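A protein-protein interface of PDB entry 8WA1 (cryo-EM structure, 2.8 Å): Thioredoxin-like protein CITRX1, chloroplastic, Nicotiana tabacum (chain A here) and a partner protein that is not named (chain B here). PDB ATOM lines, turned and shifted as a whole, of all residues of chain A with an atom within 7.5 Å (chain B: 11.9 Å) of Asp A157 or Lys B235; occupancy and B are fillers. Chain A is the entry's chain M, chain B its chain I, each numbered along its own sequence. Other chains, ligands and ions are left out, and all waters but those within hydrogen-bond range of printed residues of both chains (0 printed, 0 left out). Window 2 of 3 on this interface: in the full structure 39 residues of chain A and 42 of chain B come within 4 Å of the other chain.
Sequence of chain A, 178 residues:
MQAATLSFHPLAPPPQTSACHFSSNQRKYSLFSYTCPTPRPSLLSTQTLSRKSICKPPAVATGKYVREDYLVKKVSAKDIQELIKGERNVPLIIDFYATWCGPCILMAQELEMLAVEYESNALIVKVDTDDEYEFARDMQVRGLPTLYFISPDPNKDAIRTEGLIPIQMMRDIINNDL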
ATOM      1  N   PHE A 149       1.756  12.214  19.732  1.00  0.00           N
ATOM      2  CA  PHE A 149       2.672  12.309  20.862  1.00  0.00           C
ATOM      3  C   PHE A 149       2.251  11.291  21.915  1.00  0.00           C
ATOM      4  O   PHE A 149       1.219  11.459  22.574  1.00  0.00           O
ATOM      5  CB  PHE A 149       2.682  13.724  21.439  1.00  0.00           C
ATOM      6  CG  PHE A 149       3.306  14.745  20.533  1.00  0.00           C
ATOM      7  CD1 PHE A 149       2.542  15.421  19.598  1.00  0.00           C
ATOM      8  CD2 PHE A 149       4.658  15.030  20.618  1.00  0.00           C
ATOM      9  CE1 PHE A 149       3.114  16.362  18.764  1.00  0.00           C
ATOM     10  CE2 PHE A 149       5.237  15.969  19.787  1.00  0.00           C
ATOM     11  CZ  PHE A 149       4.464  16.636  18.859  1.00  0.00           C
ATOM     12  N   ILE A 150       3.049  10.239  22.072  1.00  0.00           N
ATOM     13  CA  ILE A 150       2.786   9.187  23.048  1.00  0.00           C
ATOM     14  C   ILE A 150       3.623   9.459  24.287  1.00  0.00           C
ATOM     15  O   ILE A 150       4.841   9.657  24.194  1.00  0.00           O
ATOM     16  CB  ILE A 150       3.098   7.796  22.469  1.00  0.00           C
ATOM     17  CG1 ILE A 150       2.323   7.567  21.171  1.00  0.00           C
ATOM     18  CG2 ILE A 150       2.767   6.714  23.485  1.00  0.00           C
ATOM     19  CD1 ILE A 150       0.823   7.607  21.337  1.00  0.00           C
ATOM     20  N   SER A 151       2.975   9.468  25.446  1.00  0.00           N
ATOM     21  CA  SER A 151       3.662   9.721  26.699  1.00  0.00           C
ATOM     22  C   SER A 151       4.347   8.455  27.201  1.00  0.00           C
ATOM     23  O   SER A 151       3.909   7.340  26.906  1.00  0.00           O
ATOM     24  CB  SER A 151       2.674  10.232  27.743  1.00  0.00           C
ATOM     25  OG  SER A 151       1.662   9.274  27.999  1.00  0.00           O
ATOM     26  N   ASP A 153       4.648   7.207  30.496  1.00  0.00           N
ATOM     27  CA  ASP A 153       3.743   6.570  31.445  1.00  0.00           C
ATOM     28  C   ASP A 153       2.497   6.192  30.725  1.00  0.00           C
ATOM     29  O   ASP A 153       1.941   7.007  30.004  1.00  0.00           O
ATOM     30  CB  ASP A 153       3.393   7.584  32.504  1.00  0.00           C
ATOM     31  CG  ASP A 153       2.119   7.252  33.250  1.00  0.00           C
ATOM     32  OD1 ASP A 153       2.103   6.265  34.013  1.00  0.00           O
ATOM     33  OD2 ASP A 153       1.132   7.993  33.089  1.00  0.00           O
ATOM     34  N   PRO A 154       2.022   4.971  30.899  1.00  0.00           N
ATOM     35  CA  PRO A 154       0.864   4.555  30.109  1.00  0.00           C
ATOM     36  C   PRO A 154      -0.517   4.928  30.633  1.00  0.00           C
ATOM     37  O   PRO A 154      -1.484   4.335  30.213  1.00  0.00           O
ATOM     38  CB  PRO A 154       0.979   3.054  30.122  1.00  0.00           C
ATOM     39  CG  PRO A 154       1.632   2.745  31.422  1.00  0.00           C
ATOM     40  CD  PRO A 154       2.626   3.846  31.626  1.00  0.00           C
ATOM     41  N   ASN A 155      -0.626   5.884  31.527  1.00  0.00           N
ATOM     42  CA  ASN A 155      -1.930   6.201  32.026  1.00  0.00           C
ATOM     43  C   ASN A 155      -2.340   7.499  31.398  1.00  0.00           C
ATOM     44  O   ASN A 155      -3.515   7.733  31.161  1.00  0.00           O
ATOM     45  CB  ASN A 155      -1.865   6.360  33.526  1.00  0.00           C
ATOM     46  CG  ASN A 155      -3.210   6.684  34.139  1.00  0.00           C
ATOM     47  OD1 ASN A 155      -4.151   5.898  34.047  1.00  0.00           O
ATOM     48  ND2 ASN A 155      -3.307   7.850  34.767  1.00  0.00           N
ATOM     49  N   LYS A 156      -1.367   8.348  31.121  1.00  0.00           N
ATOM     50  CA  LYS A 156      -1.631   9.636  30.497  1.00  0.00           C
ATOM     51  C   LYS A 156      -2.211   9.452  29.094  1.00  0.00           C
ATOM     52  O   LYS A 156      -2.120   8.383  28.482  1.00  0.00           O
ATOM     53  CB  LYS A 156      -0.356  10.476  30.441  1.00  0.00           C
ATOM     54  CG  LYS A 156       0.142  10.934  31.802  1.00  0.00           C
ATOM     55  CD  LYS A 156       1.359  11.834  31.670  1.00  0.00           C
ATOM     56  CE  LYS A 156       1.790  12.378  33.022  1.00  0.00           C
ATOM     57  NZ  LYS A 156       2.970  13.278  32.911  1.00  0.00           N
ATOM     58  N   ASP A 157      -2.814  10.522  28.586  1.00  0.00           N
ATOM     59  CA  ASP A 157      -3.484  10.513  27.295  1.00  0.00           C
ATOM     60  C   ASP A 157      -2.550  11.026  26.207  1.00  0.00           C
ATOM     61  O   ASP A 157      -1.800  11.984  26.416  1.00  0.00           O
ATOM     62  CB  ASP A 157      -4.754  11.366  27.335  1.00  0.00           C
ATOM     63  CG  ASP A 157      -5.771  10.852  28.333  1.00  0.00           C
ATOM     64  OD1 ASP A 157      -5.491   9.832  28.998  1.00  0.00           O
ATOM     65  OD2 ASP A 157      -6.851  11.466  28.453  1.00  0.00           O
ATOM     66  N   ALA A 158      -2.602  10.381  25.045  1.00  0.00           N
ATOM     67  CA  ALA A 158      -1.795  10.809  23.913  1.00  0.00           C
ATOM     68  C   ALA A 158      -2.339  12.104  23.323  1.00  0.00           C
ATOM     69  O   ALA A 158      -3.545  12.366  23.339  1.00  0.00           O
ATOM     70  CB  ALA A 158      -1.762   9.723  22.841  1.00  0.00           C
ATOM     71  N   ILE A 159      -1.431  12.920  22.794  1.00  0.00           N
ATOM     72  CA  ILE A 159      -1.775  14.182  22.154  1.00  0.00           C
ATOM     73  C   ILE A 159      -1.593  14.025  20.652  1.00  0.00           C
ATOM     74  O   ILE A 159      -0.538  13.576  20.188  1.00  0.00           O
ATOM     75  CB  ILE A 159      -0.924  15.351  22.693  1.00  0.00           C
ATOM     76  CG1 ILE A 159      -1.466  15.849  24.038  1.00  0.00           C
ATOM     77  CG2 ILE A 159      -0.873  16.493  21.685  1.00  0.00           C
ATOM     78  CD1 ILE A 159      -1.121  14.971  25.221  1.00  0.00           C
ATOM     79  N   ARG A 160      -2.624  14.388  19.895  1.00  0.00           N
ATOM     80  CA  ARG A 160      -2.587  14.350  18.441  1.00  0.00           C
ATOM     81  C   ARG A 160      -2.650  15.770  17.900  1.00  0.00           C
ATOM     82  O   ARG A 160      -3.556  16.535  18.246  1.00  0.00           O
ATOM     83  CB  ARG A 160      -3.746  13.527  17.872  1.00  0.00           C
ATOM     84  CG  ARG A 160      -3.722  13.397  16.356  1.00  0.00           C
ATOM     85  CD  ARG A 160      -5.072  12.964  15.804  1.00  0.00           C
ATOM     86  NE  ARG A 160      -6.113  13.953  16.071  1.00  0.00           N
ATOM     87  CZ  ARG A 160      -7.338  13.906  15.558  1.00  0.00           C
ATOM     88  NH1 ARG A 160      -7.682  12.918  14.744  1.00  0.00           N
ATOM     89  NH2 ARG A 160      -8.221  14.849  15.857  1.00  0.00           N
ATOM     90  N   ASP A 177       3.430  18.391  28.350  1.00  0.00           N
ATOM     91  CA  ASP A 177       2.256  17.535  28.210  1.00  0.00           C
ATOM     92  C   ASP A 177       2.615  16.062  28.364  1.00  0.00           C
ATOM     93  O   ASP A 177       1.888  15.306  29.017  1.00  0.00           O
ATOM     94  CB  ASP A 177       1.587  17.789  26.860  1.00  0.00           C
ATOM     95  CG  ASP A 177       1.155  19.232  26.688  1.00  0.00           C
ATOM     96  OD1 ASP A 177       0.802  19.871  27.701  1.00  0.00           O
ATOM     97  OD2 ASP A 177       1.172  19.729  25.543  1.00  0.00           O
ATOM     98  N   LEU A 178       3.724  15.635  27.768  1.00  0.00           N
ATOM     99  CA  LEU A 178       4.144  14.242  27.856  1.00  0.00           C
ATOM    100  C   LEU A 178       4.959  13.994  29.121  1.00  0.00           C
ATOM    101  O   LEU A 178       5.457  14.928  29.748  1.00  0.00           O
ATOM    102  CB  LEU A 178       4.955  13.844  26.624  1.00  0.00           C
ATOM    103  CG  LEU A 178       4.230  13.928  25.280  1.00  0.00           C
ATOM    104  CD1 LEU A 178       5.121  13.418  24.159  1.00  0.00           C
ATOM    105  CD2 LEU A 178       2.923  13.152  25.327  1.00  0.00           C
ATOM    106  OXT LEU A 178       5.137  12.851  29.542  1.00  0.00           O
ATOM    107  N   SER B 214      -9.538  27.466  28.351  1.00  0.00           N
ATOM    108  CA  SER B 214      -9.624  26.122  28.913  1.00  0.00           C
ATOM    109  C   SER B 214      -8.980  25.066  28.024  1.00  0.00           C
ATOM    110  O   SER B 214      -8.572  24.016  28.529  1.00  0.00           O
ATOM    111  CB  SER B 214     -11.088  25.757  29.169  1.00  0.00           C
ATOM    112  OG  SER B 214     -11.842  25.804  27.971  1.00  0.00           O
ATOM    113  N   MET B 215      -8.878  25.312  26.720  1.00  0.00           N
ATOM    114  CA  MET B 215      -8.329  24.336  25.791  1.00  0.00           C
ATOM    115  C   MET B 215      -7.259  24.986  24.925  1.00  0.00           C
ATOM    116  O   MET B 215      -7.205  26.210  24.775  1.00  0.00           O
ATOM    117  CB  MET B 215      -9.425  23.725  24.907  1.00  0.00           C
ATOM    118  N   ARG B 216      -6.403  24.142  24.351  1.00  0.00           N
ATOM    119  CA  ARG B 216      -5.287  24.576  23.521  1.00  0.00           C
ATOM    120  C   ARG B 216      -5.523  24.138  22.083  1.00  0.00           C
ATOM    121  O   ARG B 216      -5.909  22.991  21.835  1.00  0.00           O
ATOM    122  CB  ARG B 216      -3.962  24.012  24.043  1.00  0.00           C
ATOM    123  CG  ARG B 216      -4.115  23.071  25.229  1.00  0.00           C
ATOM    124  CD  ARG B 216      -2.775  22.792  25.891  1.00  0.00           C
ATOM    125  NE  ARG B 216      -1.888  22.008  25.038  1.00  0.00           N
ATOM    126  CZ  ARG B 216      -1.714  20.695  25.152  1.00  0.00           C
ATOM    127  NH1 ARG B 216      -2.365  20.017  26.086  1.00  0.00           N
ATOM    128  NH2 ARG B 216      -0.887  20.061  24.332  1.00  0.00           N
ATOM    129  N   CYS B 219      -4.324  20.431  19.427  1.00  0.00           N
ATOM    130  CA  CYS B 219      -3.997  19.190  20.120  1.00  0.00           C
ATOM    131  C   CYS B 219      -5.280  18.535  20.608  1.00  0.00           C
ATOM    132  O   CYS B 219      -6.087  19.177  21.289  1.00  0.00           O
ATOM    133  CB  CYS B 219      -3.042  19.449  21.287  1.00  0.00           C
ATOM    134  SG  CYS B 219      -3.522  20.841  22.328  1.00  0.00           S
ATOM    135  N   THR B 220      -5.463  17.265  20.259  1.00  0.00           N
ATOM    136  CA  THR B 220      -6.637  16.489  20.641  1.00  0.00           C
ATOM    137  C   THR B 220      -6.189  15.292  21.469  1.00  0.00           C
ATOM    138  O   THR B 220      -5.489  14.409  20.961  1.00  0.00           O
ATOM    139  CB  THR B 220      -7.411  16.027  19.406  1.00  0.00           C
ATOM    140  OG1 THR B 220      -7.973  17.162  18.737  1.00  0.00           O
ATOM    141  CG2 THR B 220      -8.526  15.071  19.802  1.00  0.00           C
ATOM    142  N   HIS B 221      -6.588  15.267  22.739  1.00  0.00           N
ATOM    143  CA  HIS B 221      -6.211  14.165  23.614  1.00  0.00           C
ATOM    144  C   HIS B 221      -6.925  12.885  23.203  1.00  0.00           C
ATOM    145  O   HIS B 221      -8.117  12.894  22.882  1.00  0.00           O
ATOM    146  CB  HIS B 221      -6.539  14.505  25.068  1.00  0.00           C
ATOM    147  CG  HIS B 221      -5.738  15.642  25.620  1.00  0.00           C
ATOM    148  ND1 HIS B 221      -5.804  16.025  26.942  1.00  0.00           N
ATOM    149  CD2 HIS B 221      -4.852  16.479  25.030  1.00  0.00           C
ATOM    150  CE1 HIS B 221      -4.994  17.048  27.143  1.00  0.00           C
ATOM    151  NE2 HIS B 221      -4.404  17.344  25.999  1.00  0.00           N
ATOM    152  N   MET B 222      -6.190  11.774  23.219  1.00  0.00           N
ATOM    153  CA  MET B 222      -6.738  10.478  22.848  1.00  0.00           C
ATOM    154  C   MET B 222      -6.159   9.401  23.754  1.00  0.00           C
ATOM    155  O   MET B 222      -5.261   9.649  24.562  1.00  0.00           O
ATOM    156  CB  MET B 222      -6.456  10.144  21.378  1.00  0.00           C
ATOM    157  CG  MET B 222      -7.310  10.914  20.387  1.00  0.00           C
ATOM    158  SD  MET B 222      -6.968  10.446  18.683  1.00  0.00           S
ATOM    159  CE  MET B 222      -8.181  11.437  17.818  1.00  0.00           C
ATOM    160  N   LYS B 223      -6.687   8.189  23.603  1.00  0.00           N
ATOM    161  CA  LYS B 223      -6.261   7.030  24.376  1.00  0.00           C
ATOM    162  C   LYS B 223      -6.084   5.853  23.431  1.00  0.00           C
ATOM    163  O   LYS B 223      -6.943   5.604  22.580  1.00  0.00           O
ATOM    164  CB  LYS B 223      -7.280   6.689  25.467  1.00  0.00           C
ATOM    165  CG  LYS B 223      -7.487   7.795  26.486  1.00  0.00           C
ATOM    166  CD  LYS B 223      -8.816   7.638  27.207  1.00  0.00           C
ATOM    167  CE  LYS B 223      -9.984   7.754  26.239  1.00  0.00           C
ATOM    168  NZ  LYS B 223     -11.301   7.640  26.925  1.00  0.00           N
ATOM    169  N   ILE B 224      -4.971   5.131  23.582  1.00  0.00           N
ATOM    170  CA  ILE B 224      -4.684   4.023  22.676  1.00  0.00           C
ATOM    171  C   ILE B 224      -5.662   2.876  22.897  1.00  0.00           C
ATOM    172  O   ILE B 224      -6.362   2.457  21.966  1.00  0.00           O
ATOM    173  CB  ILE B 224      -3.221   3.568  22.834  1.00  0.00           C
ATOM    174  CG1 ILE B 224      -2.627   4.077  24.152  1.00  0.00           C
ATOM    175  CG2 ILE B 224      -2.388   4.048  21.655  1.00  0.00           C
ATOM    176  CD1 ILE B 224      -2.885   3.178  25.343  1.00  0.00           C
ATOM    177  N   LYS B 225      -5.742   2.364  24.124  1.00  0.00           N
ATOM    178  CA  LYS B 225      -6.667   1.293  24.502  1.00  0.00           C
ATOM    179  C   LYS B 225      -6.553   0.098  23.550  1.00  0.00           C
ATOM    180  O   LYS B 225      -7.499  -0.289  22.865  1.00  0.00           O
ATOM    181  CB  LYS B 225      -8.106   1.814  24.554  1.00  0.00           C
ATOM    182  CG  LYS B 225      -8.323   2.959  25.529  1.00  0.00           C
ATOM    183  CD  LYS B 225      -9.798   3.307  25.634  1.00  0.00           C
ATOM    184  CE  LYS B 225     -10.399   3.584  24.266  1.00  0.00           C
ATOM    185  NZ  LYS B 225     -11.874   3.779  24.335  1.00  0.00           N
ATOM    186  N   PHE B 226      -5.356  -0.483  23.534  1.00  0.00           N
ATOM    187  CA  PHE B 226      -5.075  -1.599  22.641  1.00  0.00           C
ATOM    188  C   PHE B 226      -5.817  -2.847  23.106  1.00  0.00           C
ATOM    189  O   PHE B 226      -5.560  -3.362  24.200  1.00  0.00           O
ATOM    190  CB  PHE B 226      -3.572  -1.862  22.578  1.00  0.00           C
ATOM    191  CG  PHE B 226      -3.202  -3.080  21.779  1.00  0.00           C
ATOM    192  CD1 PHE B 226      -3.079  -3.011  20.401  1.00  0.00           C
ATOM    193  CD2 PHE B 226      -2.978  -4.295  22.406  1.00  0.00           C
ATOM    194  CE1 PHE B 226      -2.739  -4.129  19.664  1.00  0.00           C
ATOM    195  CE2 PHE B 226      -2.642  -5.417  21.674  1.00  0.00           C
ATOM    196  CZ  PHE B 226      -2.520  -5.334  20.301  1.00  0.00           C
ATOM    197  N   MET B 231      -7.327   0.782  18.639  1.00  0.00           N
ATOM    198  CA  MET B 231      -8.584   1.509  18.504  1.00  0.00           C
ATOM    199  C   MET B 231      -8.576   2.705  19.447  1.00  0.00           C
ATOM    200  O   MET B 231      -8.755   2.544  20.659  1.00  0.00           O
ATOM    201  CB  MET B 231      -9.775   0.599  18.806  1.00  0.00           C
ATOM    202  N   LYS B 232      -8.387   3.897  18.890  1.00  0.00           N
ATOM    203  CA  LYS B 232      -8.298   5.114  19.680  1.00  0.00           C
ATOM    204  C   LYS B 232      -9.685   5.697  19.943  1.00  0.00           C
ATOM    205  O   LYS B 232     -10.670   5.366  19.280  1.00  0.00           O
ATOM    206  CB  LYS B 232      -7.413   6.142  18.973  1.00  0.00           C
ATOM    207  N   VAL B 233      -9.751   6.582  20.938  1.00  0.00           N
ATOM    208  CA  VAL B 233     -10.988   7.277  21.284  1.00  0.00           C
ATOM    209  C   VAL B 233     -10.612   8.674  21.749  1.00  0.00           C
ATOM    210  O   VAL B 233      -9.522   8.896  22.277  1.00  0.00           O
ATOM    211  CB  VAL B 233     -11.787   6.511  22.370  1.00  0.00           C
ATOM    212  N   GLU B 234     -11.524   9.623  21.558  1.00  0.00           N
ATOM    213  CA  GLU B 234     -11.260  11.030  21.839  1.00  0.00           C
ATOM    214  C   GLU B 234     -11.720  11.366  23.252  1.00  0.00           C
ATOM    215  O   GLU B 234     -12.923  11.370  23.535  1.00  0.00           O
ATOM    216  CB  GLU B 234     -11.960  11.930  20.821  1.00  0.00           C
ATOM    217  CG  GLU B 234     -11.555  11.673  19.382  1.00  0.00           C
ATOM    218  CD  GLU B 234     -12.159  12.676  18.420  1.00  0.00           C
ATOM    219  OE1 GLU B 234     -12.691  13.704  18.889  1.00  0.00           O
ATOM    220  OE2 GLU B 234     -12.103  12.436  17.196  1.00  0.00           O
ATOM    221  N   LYS B 235     -10.760  11.654  24.134  1.00  0.00           N
ATOM    222  CA  LYS B 235     -11.102  12.102  25.480  1.00  0.00           C
ATOM    223  C   LYS B 235     -11.550  13.559  25.467  1.00  0.00           C
ATOM    224  O   LYS B 235     -12.613  13.899  26.001  1.00  0.00           O
ATOM    225  CB  LYS B 235      -9.909  11.909  26.416  1.00  0.00           C
ATOM    226  CG  LYS B 235     -10.181  12.296  27.861  1.00  0.00           C
ATOM    227  CD  LYS B 235     -11.277  11.433  28.468  1.00  0.00           C
ATOM    228  CE  LYS B 235     -11.507  11.777  29.932  1.00  0.00           C
ATOM    229  NZ  LYS B 235     -11.914  13.197  30.118  1.00  0.00           N
ATOM    230  N   VAL B 236     -10.750  14.435  24.857  1.00  0.00           N
ATOM    231  CA  VAL B 236     -11.082  15.843  24.697  1.00  0.00           C
ATOM    232  C   VAL B 236     -10.948  16.188  23.218  1.00  0.00           C
ATOM    233  O   VAL B 236     -10.363  15.441  22.433  1.00  0.00           O
ATOM    234  CB  VAL B 236     -10.185  16.763  25.556  1.00  0.00           C
ATOM    235  CG1 VAL B 236     -10.895  18.075  25.869  1.00  0.00           C
ATOM    236  CG2 VAL B 236      -9.763  16.064  26.840  1.00  0.00           C
ATOM    237  N   LYS B 237     -11.505  17.336  22.841  1.00  0.00           N
ATOM    238  CA  LYS B 237     -11.439  17.820  21.471  1.00  0.00           C
ATOM    239  C   LYS B 237     -10.776  19.191  21.447  1.00  0.00           C
ATOM    240  O   LYS B 237     -10.786  19.928  22.435  1.00  0.00           O
ATOM    241  CB  LYS B 237     -12.832  17.900  20.828  1.00  0.00           C
ATOM    242  CG  LYS B 237     -13.493  16.553  20.585  1.00  0.00           C
ATOM    243  CD  LYS B 237     -14.894  16.728  20.018  1.00  0.00           C
ATOM    244  CE  LYS B 237     -15.514  15.394  19.640  1.00  0.00           C
ATOM    245  NZ  LYS B 237     -14.783  14.736  18.522  1.00  0.00           N
ATOM    246  N   GLU B 238     -10.196  19.521  20.298  1.00  0.00           N
ATOM    247  CA  GLU B 238      -9.514  20.790  20.126  1.00  0.00           C
ATOM    248  C   GLU B 238     -10.519  21.924  19.950  1.00  0.00           C
ATOM    249  O   GLU B 238     -11.657  21.697  19.529  1.00  0.00           O
ATOM    250  CB  GLU B 238      -8.581  20.722  18.921  1.00  0.00           C
ATOM    251  N   PRO B 239     -10.126  23.158  20.277  1.00  0.00           N
ATOM    252  CA  PRO B 239     -11.033  24.294  20.042  1.00  0.00           C
ATOM    253  C   PRO B 239     -11.385  24.481  18.580  1.00  0.00           C
ATOM    254  O   PRO B 239     -12.470  24.992  18.272  1.00  0.00           O
ATOM    255  CB  PRO B 239     -10.242  25.492  20.587  1.00  0.00           C
ATOM    256  CG  PRO B 239      -9.251  24.904  21.529  1.00  0.00           C
ATOM    257  CD  PRO B 239      -8.888  23.571  20.958  1.00  0.00           C
ATOM    258  N   GLU B 241     -12.253  22.265  16.632  1.00  0.00           N
ATOM    259  CA  GLU B 241     -13.376  21.372  16.382  1.00  0.00           C
ATOM    260  C   GLU B 241     -14.470  21.496  17.438  1.00  0.00           C
ATOM    261  O   GLU B 241     -15.393  20.674  17.461  1.00  0.00           O
ATOM    262  CB  GLU B 241     -12.888  19.925  16.298  1.00  0.00           C
ATOM    263  CG  GLU B 241     -11.555  19.750  15.586  1.00  0.00           C
ATOM    264  CD  GLU B 241     -11.597  20.180  14.132  1.00  0.00           C
ATOM    265  OE1 GLU B 241     -12.693  20.170  13.532  1.00  0.00           O
ATOM    266  OE2 GLU B 241     -10.527  20.527  13.588  1.00  0.00           O
ATOM    267  N   ASP B 242     -14.391  22.505  18.310  1.00  0.00           N
ATOM    268  CA  ASP B 242     -15.353  22.693  19.397  1.00  0.00           C
ATOM    269  C   ASP B 242     -15.876  24.131  19.363  1.00  0.00           C
ATOM    270  O   ASP B 242     -15.312  25.035  19.983  1.00  0.00           O
ATOM    271  CB  ASP B 242     -14.728  22.362  20.753  1.00  0.00           C
ATOM    272  CG  ASP B 242     -14.697  20.873  21.034  1.00  0.00           C
ATOM    273  OD1 ASP B 242     -15.147  20.091  20.172  1.00  0.00           O
ATOM    274  OD2 ASP B 242     -14.225  20.486  22.124  1.00  0.00           O
ATOM    275  N   SER B 269     -16.569  15.762  13.508  1.00  0.00           N
ATOM    276  CA  SER B 269     -16.807  15.931  14.932  1.00  0.00           C
ATOM    277  C   SER B 269     -18.295  15.787  15.246  1.00  0.00           C
ATOM    278  O   SER B 269     -19.156  15.825  14.364  1.00  0.00           O
ATOM    279  CB  SER B 269     -16.294  17.292  15.403  1.00  0.00           C
ATOM    280  N   SER B 270     -18.594  15.626  16.539  1.00  0.00           N
ATOM    281  CA  SER B 270     -19.967  15.474  17.004  1.00  0.00           C
ATOM    282  C   SER B 270     -20.445  16.702  17.769  1.00  0.00           C
ATOM    283  O   SER B 270     -21.597  16.740  18.213  1.00  0.00           O
ATOM    284  CB  SER B 270     -20.109  14.222  17.875  1.00  0.00           C
ATOM    285  OG  SER B 270     -19.262  14.292  19.009  1.00  0.00           O
ATOM    286  N   SER B 271     -19.586  17.706  17.931  1.00  0.00           N
ATOM    287  CA  SER B 271     -19.941  18.942  18.613  1.00  0.00           C
ATOM    288  C   SER B 271     -20.021  20.134  17.672  1.00  0.00           C
ATOM    289  O   SER B 271     -20.358  21.235  18.116  1.00  0.00           O
ATOM    290  CB  SER B 271     -18.935  19.236  19.733  1.00  0.00           C
ATOM    291  OG  SER B 271     -19.263  20.437  20.411  1.00  0.00           O
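CB of Asp A157 touches O of Met B222, at 3.3 Å.
Asp A157 touches Lys B223.
Asp A157 touches Lys B235.
Ala A158 touches Thr B220.
His B221 touches Ala A158.
Ile A159 touches Cys B219 (CG2 to CB, 3.7 Å).
Ile A159 touches Thr B220.
CD2 of His B221 touches CG1 of Ile A159, 3.6 Å away.
Cys B219 touches Arg A160.
Arg A160 touches Met B222 (NH1 to CE, 3.4 Å).
No residue of chain B comes within 4 Å of Ile A150.
No residue of chain B comes within 4 Å of Lys A156.
Asp A157 touches just these residues of chain B: Met B222 (3.3 Å), Lys B223 (3.8 Å) and Lys B235 (3.5 Å).
Of chain B, only Thr B220, His B221 and Met B222 come within 4 Å of Ala A158.
Ile A159 touches just these residues of chain B: Cys B219 (3.7 Å), Thr B220 (3.9 Å) and His B221 (3.6 Å).
Printed residues of chain B within 4 Å of Arg A160: Cys B219 (3.3 Å), Thr B220 (2.9 Å) and Met B222 (3.4 Å).
Of the printed residues of chain B, Asp A177 touches Arg B216 (2.4 Å).
Printed residues of chain A within 4 Å of Cys B219: Ile A159 (3.7 Å) and Arg A160 (3.3 Å).
Of the printed residues of chain A, Met B222 touches Asp A157 (3.3 Å), Ala A158 (2.7 Å) and Arg A160 (3.4 Å).
The nearest residue of chain B that does not touch Asp A157 is His B221 (4.3 Å).
O of Ala A158 is in hydrogen-bond range of N of Met B222 (2.7 Å).
The backbone NH (N) of Thr B220 is in hydrogen-bond range of the backbone carbonyl oxygen (O) of Arg A160, 2.9 Å away.
The guanidinium group of Arg B216 is in salt-bridge range of the side-chain carboxylate of Asp A177.
The backbone carbonyl oxygen (O) of Ile A159 sits at hydrogen-bond distance from the backbone NH (N) of Phe A149.
The backbone carbonyl oxygen (O) of Arg B216 sits at hydrogen-bond distance from the side-chain sulfur (SG) of Cys B219, at 3.3 Å.
NH1 of Arg B216 sits at hydrogen-bond distance from NE2 of His B221.
The backbone NH (N) of Lys B235 is in hydrogen-bond range of the backbone carbonyl oxygen (O) of His B221, 3.2 Å away.
O of Val B233 sits at hydrogen-bond distance from N of Lys B223 (3.2 Å).
Printed residues of chain A that touch a printed residue of chain B: Asp A157, Ala A158, Ile A159, Arg A160 and Asp A177.
Hydrophobic or aromatic side chains of chain A that line the printed part of chain B: Ala A158 and Ile A159.
Of the 25 printed residues of chain B, 7 touch a printed residue of chain A.
Hydrophobic or aromatic side chains of chain B that line the printed part of chain A: His B221 and Met B222.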
